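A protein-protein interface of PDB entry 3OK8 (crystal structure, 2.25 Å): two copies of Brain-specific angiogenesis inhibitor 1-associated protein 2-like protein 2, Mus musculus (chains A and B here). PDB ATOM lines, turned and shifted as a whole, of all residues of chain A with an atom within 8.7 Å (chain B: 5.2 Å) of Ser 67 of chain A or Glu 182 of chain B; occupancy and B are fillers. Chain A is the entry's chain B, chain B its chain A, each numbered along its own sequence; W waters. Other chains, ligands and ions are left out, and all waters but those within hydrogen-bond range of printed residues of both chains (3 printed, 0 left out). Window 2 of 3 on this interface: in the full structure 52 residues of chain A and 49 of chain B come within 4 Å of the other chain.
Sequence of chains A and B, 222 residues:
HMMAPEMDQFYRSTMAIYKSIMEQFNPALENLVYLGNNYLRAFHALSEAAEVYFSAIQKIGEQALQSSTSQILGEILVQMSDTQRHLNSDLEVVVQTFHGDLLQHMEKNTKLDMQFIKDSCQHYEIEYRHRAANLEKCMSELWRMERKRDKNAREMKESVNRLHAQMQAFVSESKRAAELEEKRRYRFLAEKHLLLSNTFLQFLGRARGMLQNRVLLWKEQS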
ATOM      1  N   ILE A  60      15.423   8.603 -15.989  1.00  0.00           N
ATOM      2  CA  ILE A  60      15.063   8.933 -14.625  1.00  0.00           C
ATOM      3  C   ILE A  60      15.090   7.670 -13.780  1.00  0.00           C
ATOM      4  O   ILE A  60      15.595   7.679 -12.653  1.00  0.00           O
ATOM      5  CB  ILE A  60      13.696   9.644 -14.607  1.00  0.00           C
ATOM      6  CG1 ILE A  60      13.852  11.028 -15.251  1.00  0.00           C
ATOM      7  CG2 ILE A  60      13.117   9.734 -13.202  1.00  0.00           C
ATOM      8  CD1 ILE A  60      12.723  11.988 -14.984  1.00  0.00           C
ATOM      9  N   GLY A  61      14.577   6.581 -14.347  1.00  0.00           N
ATOM     10  CA  GLY A  61      14.609   5.287 -13.704  1.00  0.00           C
ATOM     11  C   GLY A  61      16.039   4.864 -13.428  1.00  0.00           C
ATOM     12  O   GLY A  61      16.333   4.291 -12.380  1.00  0.00           O
ATOM     13  N   GLU A  62      16.928   5.164 -14.369  1.00  0.00           N
ATOM     14  CA  GLU A  62      18.340   4.812 -14.259  1.00  0.00           C
ATOM     15  C   GLU A  62      19.048   5.679 -13.211  1.00  0.00           C
ATOM     16  O   GLU A  62      20.025   5.255 -12.624  1.00  0.00           O
ATOM     17  CB  GLU A  62      19.032   4.925 -15.635  1.00  0.00           C
ATOM     18  CG  GLU A  62      18.668   3.800 -16.620  1.00  0.00           C
ATOM     19  CD  GLU A  62      18.965   4.156 -18.082  1.00  0.00           C
ATOM     20  OE1 GLU A  62      19.453   5.282 -18.341  1.00  0.00           O
ATOM     21  OE2 GLU A  62      18.710   3.309 -18.974  1.00  0.00           O
ATOM     22  N   GLN A  63      18.550   6.892 -12.994  1.00  0.00           N
ATOM     23  CA  GLN A  63      19.042   7.763 -11.935  1.00  0.00           C
ATOM     24  C   GLN A  63      18.524   7.287 -10.565  1.00  0.00           C
ATOM     25  O   GLN A  63      19.241   7.352  -9.576  1.00  0.00           O
ATOM     26  CB  GLN A  63      18.689   9.237 -12.221  1.00  0.00           C
ATOM     27  CG  GLN A  63      19.271   9.740 -13.539  1.00  0.00           C
ATOM     28  CD  GLN A  63      18.868  11.171 -13.917  1.00  0.00           C
ATOM     29  OE1 GLN A  63      17.687  11.529 -13.933  1.00  0.00           O
ATOM     30  NE2 GLN A  63      19.863  11.989 -14.248  1.00  0.00           N
ATOM     31  N   ALA A  64      17.290   6.776 -10.518  1.00  0.00           N
ATOM     32  CA  ALA A  64      16.729   6.216  -9.292  1.00  0.00           C
ATOM     33  C   ALA A  64      17.427   4.903  -8.942  1.00  0.00           C
ATOM     34  O   ALA A  64      17.713   4.628  -7.771  1.00  0.00           O
ATOM     35  CB  ALA A  64      15.225   6.015  -9.420  1.00  0.00           C
ATOM     36  N   LEU A  65      17.724   4.106  -9.962  1.00  0.00           N
ATOM     37  CA  LEU A  65      18.512   2.892  -9.769  1.00  0.00           C
ATOM     38  C   LEU A  65      19.890   3.139  -9.128  1.00  0.00           C
ATOM     39  O   LEU A  65      20.506   2.201  -8.602  1.00  0.00           O
ATOM     40  CB  LEU A  65      18.667   2.137 -11.089  1.00  0.00           C
ATOM     41  CG  LEU A  65      17.443   1.319 -11.512  1.00  0.00           C
ATOM     42  CD1 LEU A  65      17.503   0.956 -12.988  1.00  0.00           C
ATOM     43  CD2 LEU A  65      17.313   0.076 -10.649  1.00  0.00           C
ATOM     44  N   GLN A  66      20.370   4.385  -9.169  1.00  0.00           N
ATOM     45  CA  GLN A  66      21.668   4.736  -8.578  1.00  0.00           C
ATOM     46  C   GLN A  66      21.551   5.565  -7.293  1.00  0.00           C
ATOM     47  O   GLN A  66      22.534   6.139  -6.830  1.00  0.00           O
ATOM     48  CB  GLN A  66      22.551   5.478  -9.592  1.00  0.00           C
ATOM     49  CG  GLN A  66      22.932   4.662 -10.817  1.00  0.00           C
ATOM     50  CD  GLN A  66      23.601   3.345 -10.464  1.00  0.00           C
ATOM     51  OE1 GLN A  66      23.323   2.317 -11.078  1.00  0.00           O
ATOM     52  NE2 GLN A  66      24.486   3.370  -9.470  1.00  0.00           N
ATOM     53  N   SER A  67      20.349   5.639  -6.724  1.00  0.00           N
ATOM     54  CA  SER A  67      20.163   6.320  -5.444  1.00  0.00           C
ATOM     55  C   SER A  67      20.311   5.304  -4.317  1.00  0.00           C
ATOM     56  O   SER A  67      20.542   4.115  -4.568  1.00  0.00           O
ATOM     57  CB  SER A  67      18.792   6.990  -5.357  1.00  0.00           C
ATOM     58  OG  SER A  67      17.772   6.027  -5.135  1.00  0.00           O
ATOM     59  N   SER A  68      20.178   5.770  -3.081  1.00  0.00           N
ATOM     60  CA  SER A  68      20.283   4.891  -1.923  1.00  0.00           C
ATOM     61  C   SER A  68      19.004   4.097  -1.630  1.00  0.00           C
ATOM     62  O   SER A  68      19.075   2.918  -1.289  1.00  0.00           O
ATOM     63  CB  SER A  68      20.703   5.680  -0.679  1.00  0.00           C
ATOM     64  OG  SER A  68      19.751   6.679  -0.353  1.00  0.00           O
ATOM     65  N   THR A  69      17.836   4.725  -1.754  1.00  0.00           N
ATOM     66  CA  THR A  69      16.596   4.052  -1.359  1.00  0.00           C
ATOM     67  C   THR A  69      15.536   3.913  -2.470  1.00  0.00           C
ATOM     68  O   THR A  69      14.514   3.258  -2.268  1.00  0.00           O
ATOM     69  CB  THR A  69      15.949   4.745  -0.154  1.00  0.00           C
ATOM     70  OG1 THR A  69      15.668   6.102  -0.500  1.00  0.00           O
ATOM     71  CG2 THR A  69      16.891   4.699   1.097  1.00  0.00           C
ATOM     72  N   SER A  70      15.768   4.521  -3.632  1.00  0.00           N
ATOM     73  CA  SER A  70      14.760   4.520  -4.691  1.00  0.00           C
ATOM     74  C   SER A  70      15.020   3.537  -5.822  1.00  0.00           C
ATOM     75  O   SER A  70      14.592   3.788  -6.954  1.00  0.00           O
ATOM     76  CB  SER A  70      14.617   5.918  -5.286  1.00  0.00           C
ATOM     77  OG  SER A  70      14.061   6.816  -4.351  1.00  0.00           O
ATOM     78  N   GLN A  71      15.705   2.434  -5.534  1.00  0.00           N
ATOM     79  CA  GLN A  71      16.043   1.480  -6.577  1.00  0.00           C
ATOM     80  C   GLN A  71      14.824   0.755  -7.140  1.00  0.00           C
ATOM     81  O   GLN A  71      14.750   0.509  -8.344  1.00  0.00           O
ATOM     82  CB  GLN A  71      17.088   0.499  -6.066  1.00  0.00           C
ATOM     83  CG  GLN A  71      18.306   1.195  -5.446  1.00  0.00           C
ATOM     84  CD  GLN A  71      18.358   1.101  -3.921  1.00  0.00           C
ATOM     85  OE1 GLN A  71      19.373   0.690  -3.374  1.00  0.00           O
ATOM     86  NE2 GLN A  71      17.271   1.474  -3.235  1.00  0.00           N
ATOM     87  N   ILE A  72      13.872   0.429  -6.279  1.00  0.00           N
ATOM     88  CA  ILE A  72      12.695  -0.303  -6.714  1.00  0.00           C
ATOM     89  C   ILE A  72      11.774   0.540  -7.607  1.00  0.00           C
ATOM     90  O   ILE A  72      11.276   0.055  -8.628  1.00  0.00           O
ATOM     91  CB  ILE A  72      11.959  -0.918  -5.508  1.00  0.00           C
ATOM     92  CG1 ILE A  72      12.780  -2.098  -4.974  1.00  0.00           C
ATOM     93  CG2 ILE A  72      10.539  -1.294  -5.877  1.00  0.00           C
ATOM     94  CD1 ILE A  72      12.072  -2.954  -3.957  1.00  0.00           C
ATOM     95  N   LEU A  73      11.585   1.806  -7.241  1.00  0.00           N
ATOM     96  CA  LEU A  73      10.837   2.763  -8.054  1.00  0.00           C
ATOM     97  C   LEU A  73      11.532   3.035  -9.382  1.00  0.00           C
ATOM     98  O   LEU A  73      10.880   3.278 -10.397  1.00  0.00           O
ATOM     99  CB  LEU A  73      10.649   4.074  -7.296  1.00  0.00           C
ATOM    100  CG  LEU A  73       9.811   3.945  -6.025  1.00  0.00           C
ATOM    101  CD1 LEU A  73       9.969   5.177  -5.148  1.00  0.00           C
ATOM    102  CD2 LEU A  73       8.354   3.710  -6.387  1.00  0.00           C
ATOM    103  N   GLY A  74      12.858   2.997  -9.361  1.00  0.00           N
ATOM    104  CA  GLY A  74      13.647   3.216 -10.553  1.00  0.00           C
ATOM    105  C   GLY A  74      13.555   2.025 -11.471  1.00  0.00           C
ATOM    106  O   GLY A  74      13.534   2.171 -12.690  1.00  0.00           O
ATOM    107  N   ILE B  17      22.251  14.966  -2.393  1.00  0.00           N
ATOM    108  CA  ILE B  17      20.871  14.559  -2.598  1.00  0.00           C
ATOM    109  C   ILE B  17      19.962  15.728  -2.954  1.00  0.00           C
ATOM    110  O   ILE B  17      19.192  15.650  -3.912  1.00  0.00           O
ATOM    111  CB  ILE B  17      20.315  13.855  -1.369  1.00  0.00           C
ATOM    112  CG1 ILE B  17      20.986  12.494  -1.207  1.00  0.00           C
ATOM    113  CG2 ILE B  17      18.795  13.722  -1.488  1.00  0.00           C
ATOM    114  CD1 ILE B  17      20.606  11.772   0.074  1.00  0.00           C
ATOM    115  N   SER B  20      20.848  16.562  -6.363  1.00  0.00           N
ATOM    116  CA  SER B  20      20.286  15.642  -7.356  1.00  0.00           C
ATOM    117  C   SER B  20      18.866  16.060  -7.691  1.00  0.00           C
ATOM    118  O   SER B  20      18.436  16.007  -8.842  1.00  0.00           O
ATOM    119  CB  SER B  20      20.270  14.203  -6.838  1.00  0.00           C
ATOM    120  OG  SER B  20      21.485  13.535  -7.107  1.00  0.00           O
ATOM    121  N   ILE B  21      18.129  16.464  -6.664  1.00  0.00           N
ATOM    122  CA  ILE B  21      16.744  16.863  -6.842  1.00  0.00           C
ATOM    123  C   ILE B  21      16.652  18.156  -7.652  1.00  0.00           C
ATOM    124  O   ILE B  21      15.844  18.268  -8.554  1.00  0.00           O
ATOM    125  CB  ILE B  21      16.028  17.039  -5.480  1.00  0.00           C
ATOM    126  CG1 ILE B  21      15.929  15.696  -4.747  1.00  0.00           C
ATOM    127  CG2 ILE B  21      14.651  17.678  -5.662  1.00  0.00           C
ATOM    128  CD1 ILE B  21      15.382  15.816  -3.324  1.00  0.00           C
ATOM    129  N   ALA B 178      16.243  13.813   3.711  1.00  0.00           N
ATOM    130  CA  ALA B 178      16.565  14.204   2.340  1.00  0.00           C
ATOM    131  C   ALA B 178      16.433  13.030   1.374  1.00  0.00           C
ATOM    132  O   ALA B 178      15.955  13.198   0.242  1.00  0.00           O
ATOM    133  CB  ALA B 178      17.955  14.802   2.264  1.00  0.00           C
ATOM    134  N   GLU B 179      16.883  11.853   1.814  1.00  0.00           N
ATOM    135  CA  GLU B 179      16.682  10.612   1.068  1.00  0.00           C
ATOM    136  C   GLU B 179      15.206  10.387   0.811  1.00  0.00           C
ATOM    137  O   GLU B 179      14.798  10.005  -0.293  1.00  0.00           O
ATOM    138  CB  GLU B 179      17.199   9.411   1.862  1.00  0.00           C
ATOM    139  CG  GLU B 179      18.674   9.101   1.702  1.00  0.00           C
ATOM    140  CD  GLU B 179      19.122   7.953   2.607  1.00  0.00           C
ATOM    141  OE1 GLU B 179      18.572   7.819   3.732  1.00  0.00           O
ATOM    142  OE2 GLU B 179      20.022   7.186   2.198  1.00  0.00           O
ATOM    143  N   LEU B 180      14.411  10.592   1.857  1.00  0.00           N
ATOM    144  CA  LEU B 180      12.979  10.376   1.785  1.00  0.00           C
ATOM    145  C   LEU B 180      12.335  11.246   0.702  1.00  0.00           C
ATOM    146  O   LEU B 180      11.590  10.743  -0.134  1.00  0.00           O
ATOM    147  CB  LEU B 180      12.325  10.628   3.141  1.00  0.00           C
ATOM    148  CG  LEU B 180      10.883  10.149   3.316  1.00  0.00           C
ATOM    149  CD1 LEU B 180      10.689   8.723   2.811  1.00  0.00           C
ATOM    150  CD2 LEU B 180      10.477  10.245   4.773  1.00  0.00           C
ATOM    151  N   GLU B 181      12.628  12.545   0.738  1.00  0.00           N
ATOM    152  CA  GLU B 181      12.135  13.501  -0.250  1.00  0.00           C
ATOM    153  C   GLU B 181      12.458  13.064  -1.674  1.00  0.00           C
ATOM    154  O   GLU B 181      11.633  13.191  -2.586  1.00  0.00           O
ATOM    155  CB  GLU B 181      12.752  14.876   0.006  1.00  0.00           C
ATOM    156  CG  GLU B 181      12.274  15.529   1.290  1.00  0.00           C
ATOM    157  CD  GLU B 181      10.775  15.793   1.298  1.00  0.00           C
ATOM    158  OE1 GLU B 181      10.091  15.277   2.208  1.00  0.00           O
ATOM    159  OE2 GLU B 181      10.279  16.518   0.403  1.00  0.00           O
ATOM    160  N   GLU B 182      13.675  12.576  -1.865  1.00  0.00           N
ATOM    161  CA  GLU B 182      14.091  12.097  -3.167  1.00  0.00           C
ATOM    162  C   GLU B 182      13.190  10.954  -3.586  1.00  0.00           C
ATOM    163  O   GLU B 182      12.649  10.948  -4.701  1.00  0.00           O
ATOM    164  CB  GLU B 182      15.535  11.626  -3.116  1.00  0.00           C
ATOM    165  CG  GLU B 182      16.044  11.013  -4.397  1.00  0.00           C
ATOM    166  CD  GLU B 182      17.521  10.724  -4.319  1.00  0.00           C
ATOM    167  OE1 GLU B 182      17.897   9.743  -3.643  1.00  0.00           O
ATOM    168  OE2 GLU B 182      18.308  11.493  -4.919  1.00  0.00           O
ATOM    169  N   LYS B 183      13.023   9.986  -2.693  1.00  0.00           N
ATOM    170  CA  LYS B 183      12.176   8.829  -2.990  1.00  0.00           C
ATOM    171  C   LYS B 183      10.727   9.231  -3.250  1.00  0.00           C
ATOM    172  O   LYS B 183      10.060   8.660  -4.112  1.00  0.00           O
ATOM    173  CB  LYS B 183      12.236   7.788  -1.873  1.00  0.00           C
ATOM    174  CG  LYS B 183      11.453   6.518  -2.178  1.00  0.00           C
ATOM    175  CD  LYS B 183      11.624   5.434  -1.105  1.00  0.00           C
ATOM    176  CE  LYS B 183      11.258   4.061  -1.645  1.00  0.00           C
ATOM    177  NZ  LYS B 183      11.386   2.963  -0.642  1.00  0.00           N
ATOM    178  N   ARG B 184      10.242  10.218  -2.506  1.00  0.00           N
ATOM    179  CA  ARG B 184       8.864  10.653  -2.655  1.00  0.00           C
ATOM    180  C   ARG B 184       8.597  11.173  -4.063  1.00  0.00           C
ATOM    181  O   ARG B 184       7.506  10.988  -4.611  1.00  0.00           O
ATOM    182  CB  ARG B 184       8.531  11.713  -1.614  1.00  0.00           C
ATOM    183  CG  ARG B 184       8.164  11.105  -0.271  1.00  0.00           C
ATOM    184  CD  ARG B 184       8.117  12.139   0.843  1.00  0.00           C
ATOM    185  NE  ARG B 184       7.436  11.603   2.019  1.00  0.00           N
ATOM    186  CZ  ARG B 184       7.404  12.197   3.213  1.00  0.00           C
ATOM    187  NH1 ARG B 184       6.753  11.631   4.226  1.00  0.00           N
ATOM    188  NH2 ARG B 184       8.012  13.359   3.401  1.00  0.00           N
ATOM    189  N   ARG B 185       9.607  11.811  -4.646  1.00  0.00           N
ATOM    190  CA  ARG B 185       9.497  12.368  -5.990  1.00  0.00           C
ATOM    191  C   ARG B 185       9.626  11.310  -7.087  1.00  0.00           C
ATOM    192  O   ARG B 185       8.922  11.382  -8.093  1.00  0.00           O
ATOM    193  CB  ARG B 185      10.468  13.541  -6.165  1.00  0.00           C
ATOM    194  CG  ARG B 185       9.961  14.798  -5.474  1.00  0.00           C
ATOM    195  CD  ARG B 185      11.055  15.691  -4.902  1.00  0.00           C
ATOM    196  NE  ARG B 185      10.468  16.771  -4.111  1.00  0.00           N
ATOM    197  CZ  ARG B 185      10.059  16.636  -2.851  1.00  0.00           C
ATOM    198  NH1 ARG B 185       9.529  17.664  -2.201  1.00  0.00           N
ATOM    199  NH2 ARG B 185      10.181  15.469  -2.230  1.00  0.00           N
ATOM    200  N   TYR B 186      10.486  10.313  -6.911  1.00  0.00           N
ATOM    201  CA  TYR B 186      10.444   9.179  -7.836  1.00  0.00           C
ATOM    202  C   TYR B 186       9.087   8.472  -7.793  1.00  0.00           C
ATOM    203  O   TYR B 186       8.473   8.190  -8.836  1.00  0.00           O
ATOM    204  CB  TYR B 186      11.556   8.183  -7.560  1.00  0.00           C
ATOM    205  CG  TYR B 186      12.904   8.686  -8.009  1.00  0.00           C
ATOM    206  CD1 TYR B 186      13.169   8.870  -9.354  1.00  0.00           C
ATOM    207  CD2 TYR B 186      13.915   8.983  -7.090  1.00  0.00           C
ATOM    208  CE1 TYR B 186      14.385   9.330  -9.791  1.00  0.00           C
ATOM    209  CE2 TYR B 186      15.149   9.452  -7.521  1.00  0.00           C
ATOM    210  CZ  TYR B 186      15.375   9.620  -8.882  1.00  0.00           C
ATOM    211  OH  TYR B 186      16.575  10.079  -9.345  1.00  0.00           O
HETATM  212  O   HOH W   1      20.309   8.571  -2.454  1.00  0.00           O
HETATM  213  O   HOH W   2      16.743  11.931 -11.480  1.00  0.00           O
HETATM  214  O   HOH W   3      16.455   7.416  -2.634  1.00  0.00           O
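OG of Ser 68 of chain A sits at hydrogen-bond distance from OE2 of Glu 179 of chain B, 2.6 Å away.
The backbone carbonyl oxygen (O) of Ala 64 of chain A lies within hydrogen-bond range of the side-chain hydroxyl (OG) of Ser 67 of chain A (3.0 Å).
The side-chain hydroxyl (OG) of Ser 67 of chain A lies within hydrogen-bond range of the backbone NH (N) of Ser 70 of chain A (2.9 Å).
The backbone carbonyl oxygen of Ser 68 of chain A sits at hydrogen-bond distance from the side-chain amide nitrogen of Gln 71 of chain A (3.0 Å).
The backbone carbonyl oxygen (O) of Thr 69 of chain A sits close to the side-chain amide nitrogen (NE2) of Gln 71 of chain A (3.4 Å).
Tyr 186 of chain B touches Ile 60 of chain A (CE1 to O, 3.5 Å).
Gln 63 of chain A touches Tyr 186 of chain B.
CB of Ala 64 of chain A touches CE1 of Tyr 186 of chain B (3.4 Å).
CB of Ser 67 of chain A touches OE1 of Glu 182 of chain B (3.4 Å).
O of Thr 69 of chain A touches CE of Lys 183 of chain B (3.4 Å).
Ser 70 of chain A touches Lys 183 of chain B (OG to CA, 3.1 Å).
OG of Ser 70 of chain A touches CD2 of Tyr 186 of chain B, 3.5 Å away.
Leu 73 of chain A touches Lys 183 of chain B (CD1 to CG, 3.6 Å).
Ser 67 of chain A touches just one residue of chain B: Glu 182.
Printed residues of chain A within 4 Å of Glu 179 of chain B: Ser 68 (2.6 Å).
Glu 181 of chain B touches none of the printed residues of chain A.
Glu 182 of chain B touches one residue of chain A.
Of the printed residues of chain A, Tyr 186 of chain B touches Ile 60, Gln 63, Ala 64 and Ser 70.
The nearest residue of chain A that does not touch Glu 182 of chain B is Ser 70 of chain A (4.3 Å).
Of the 15 printed residues of chain A, 8 touch a printed residue of chain B.
Of the 12 printed residues of chain B, 4 touch a printed residue of chain A.
Printed residues of chain B that touch a printed residue of chain A: Glu 179, Glu 182, Lys 183 and Tyr 186.
Hydrophobic or aromatic side chains of chain B that line the printed part of chain A: Tyr 186.
No position is printed for both chains.
Water W3 lies within hydrogen-bond range of the side-chain hydroxyl of Thr 69 of chain A (2.6 Å), the side-chain carboxylate of Glu 182 of chain B (2.9 Å), the side-chain hydroxyl of Ser 70 of chain A (3.0 Å) and the side-chain hydroxyl of Ser 67 of chain A (3.1 Å).
Water W2 bridges OE1 of Gln 63 of chain A and OH of Tyr 186 of chain B.
Water W1 lies within hydrogen-bond range of the backbone NH (N) of Ser 68 of chain A (2.9 Å) and the side-chain carboxylate (OE1) of Glu 182 of chain B (2.9 Å).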
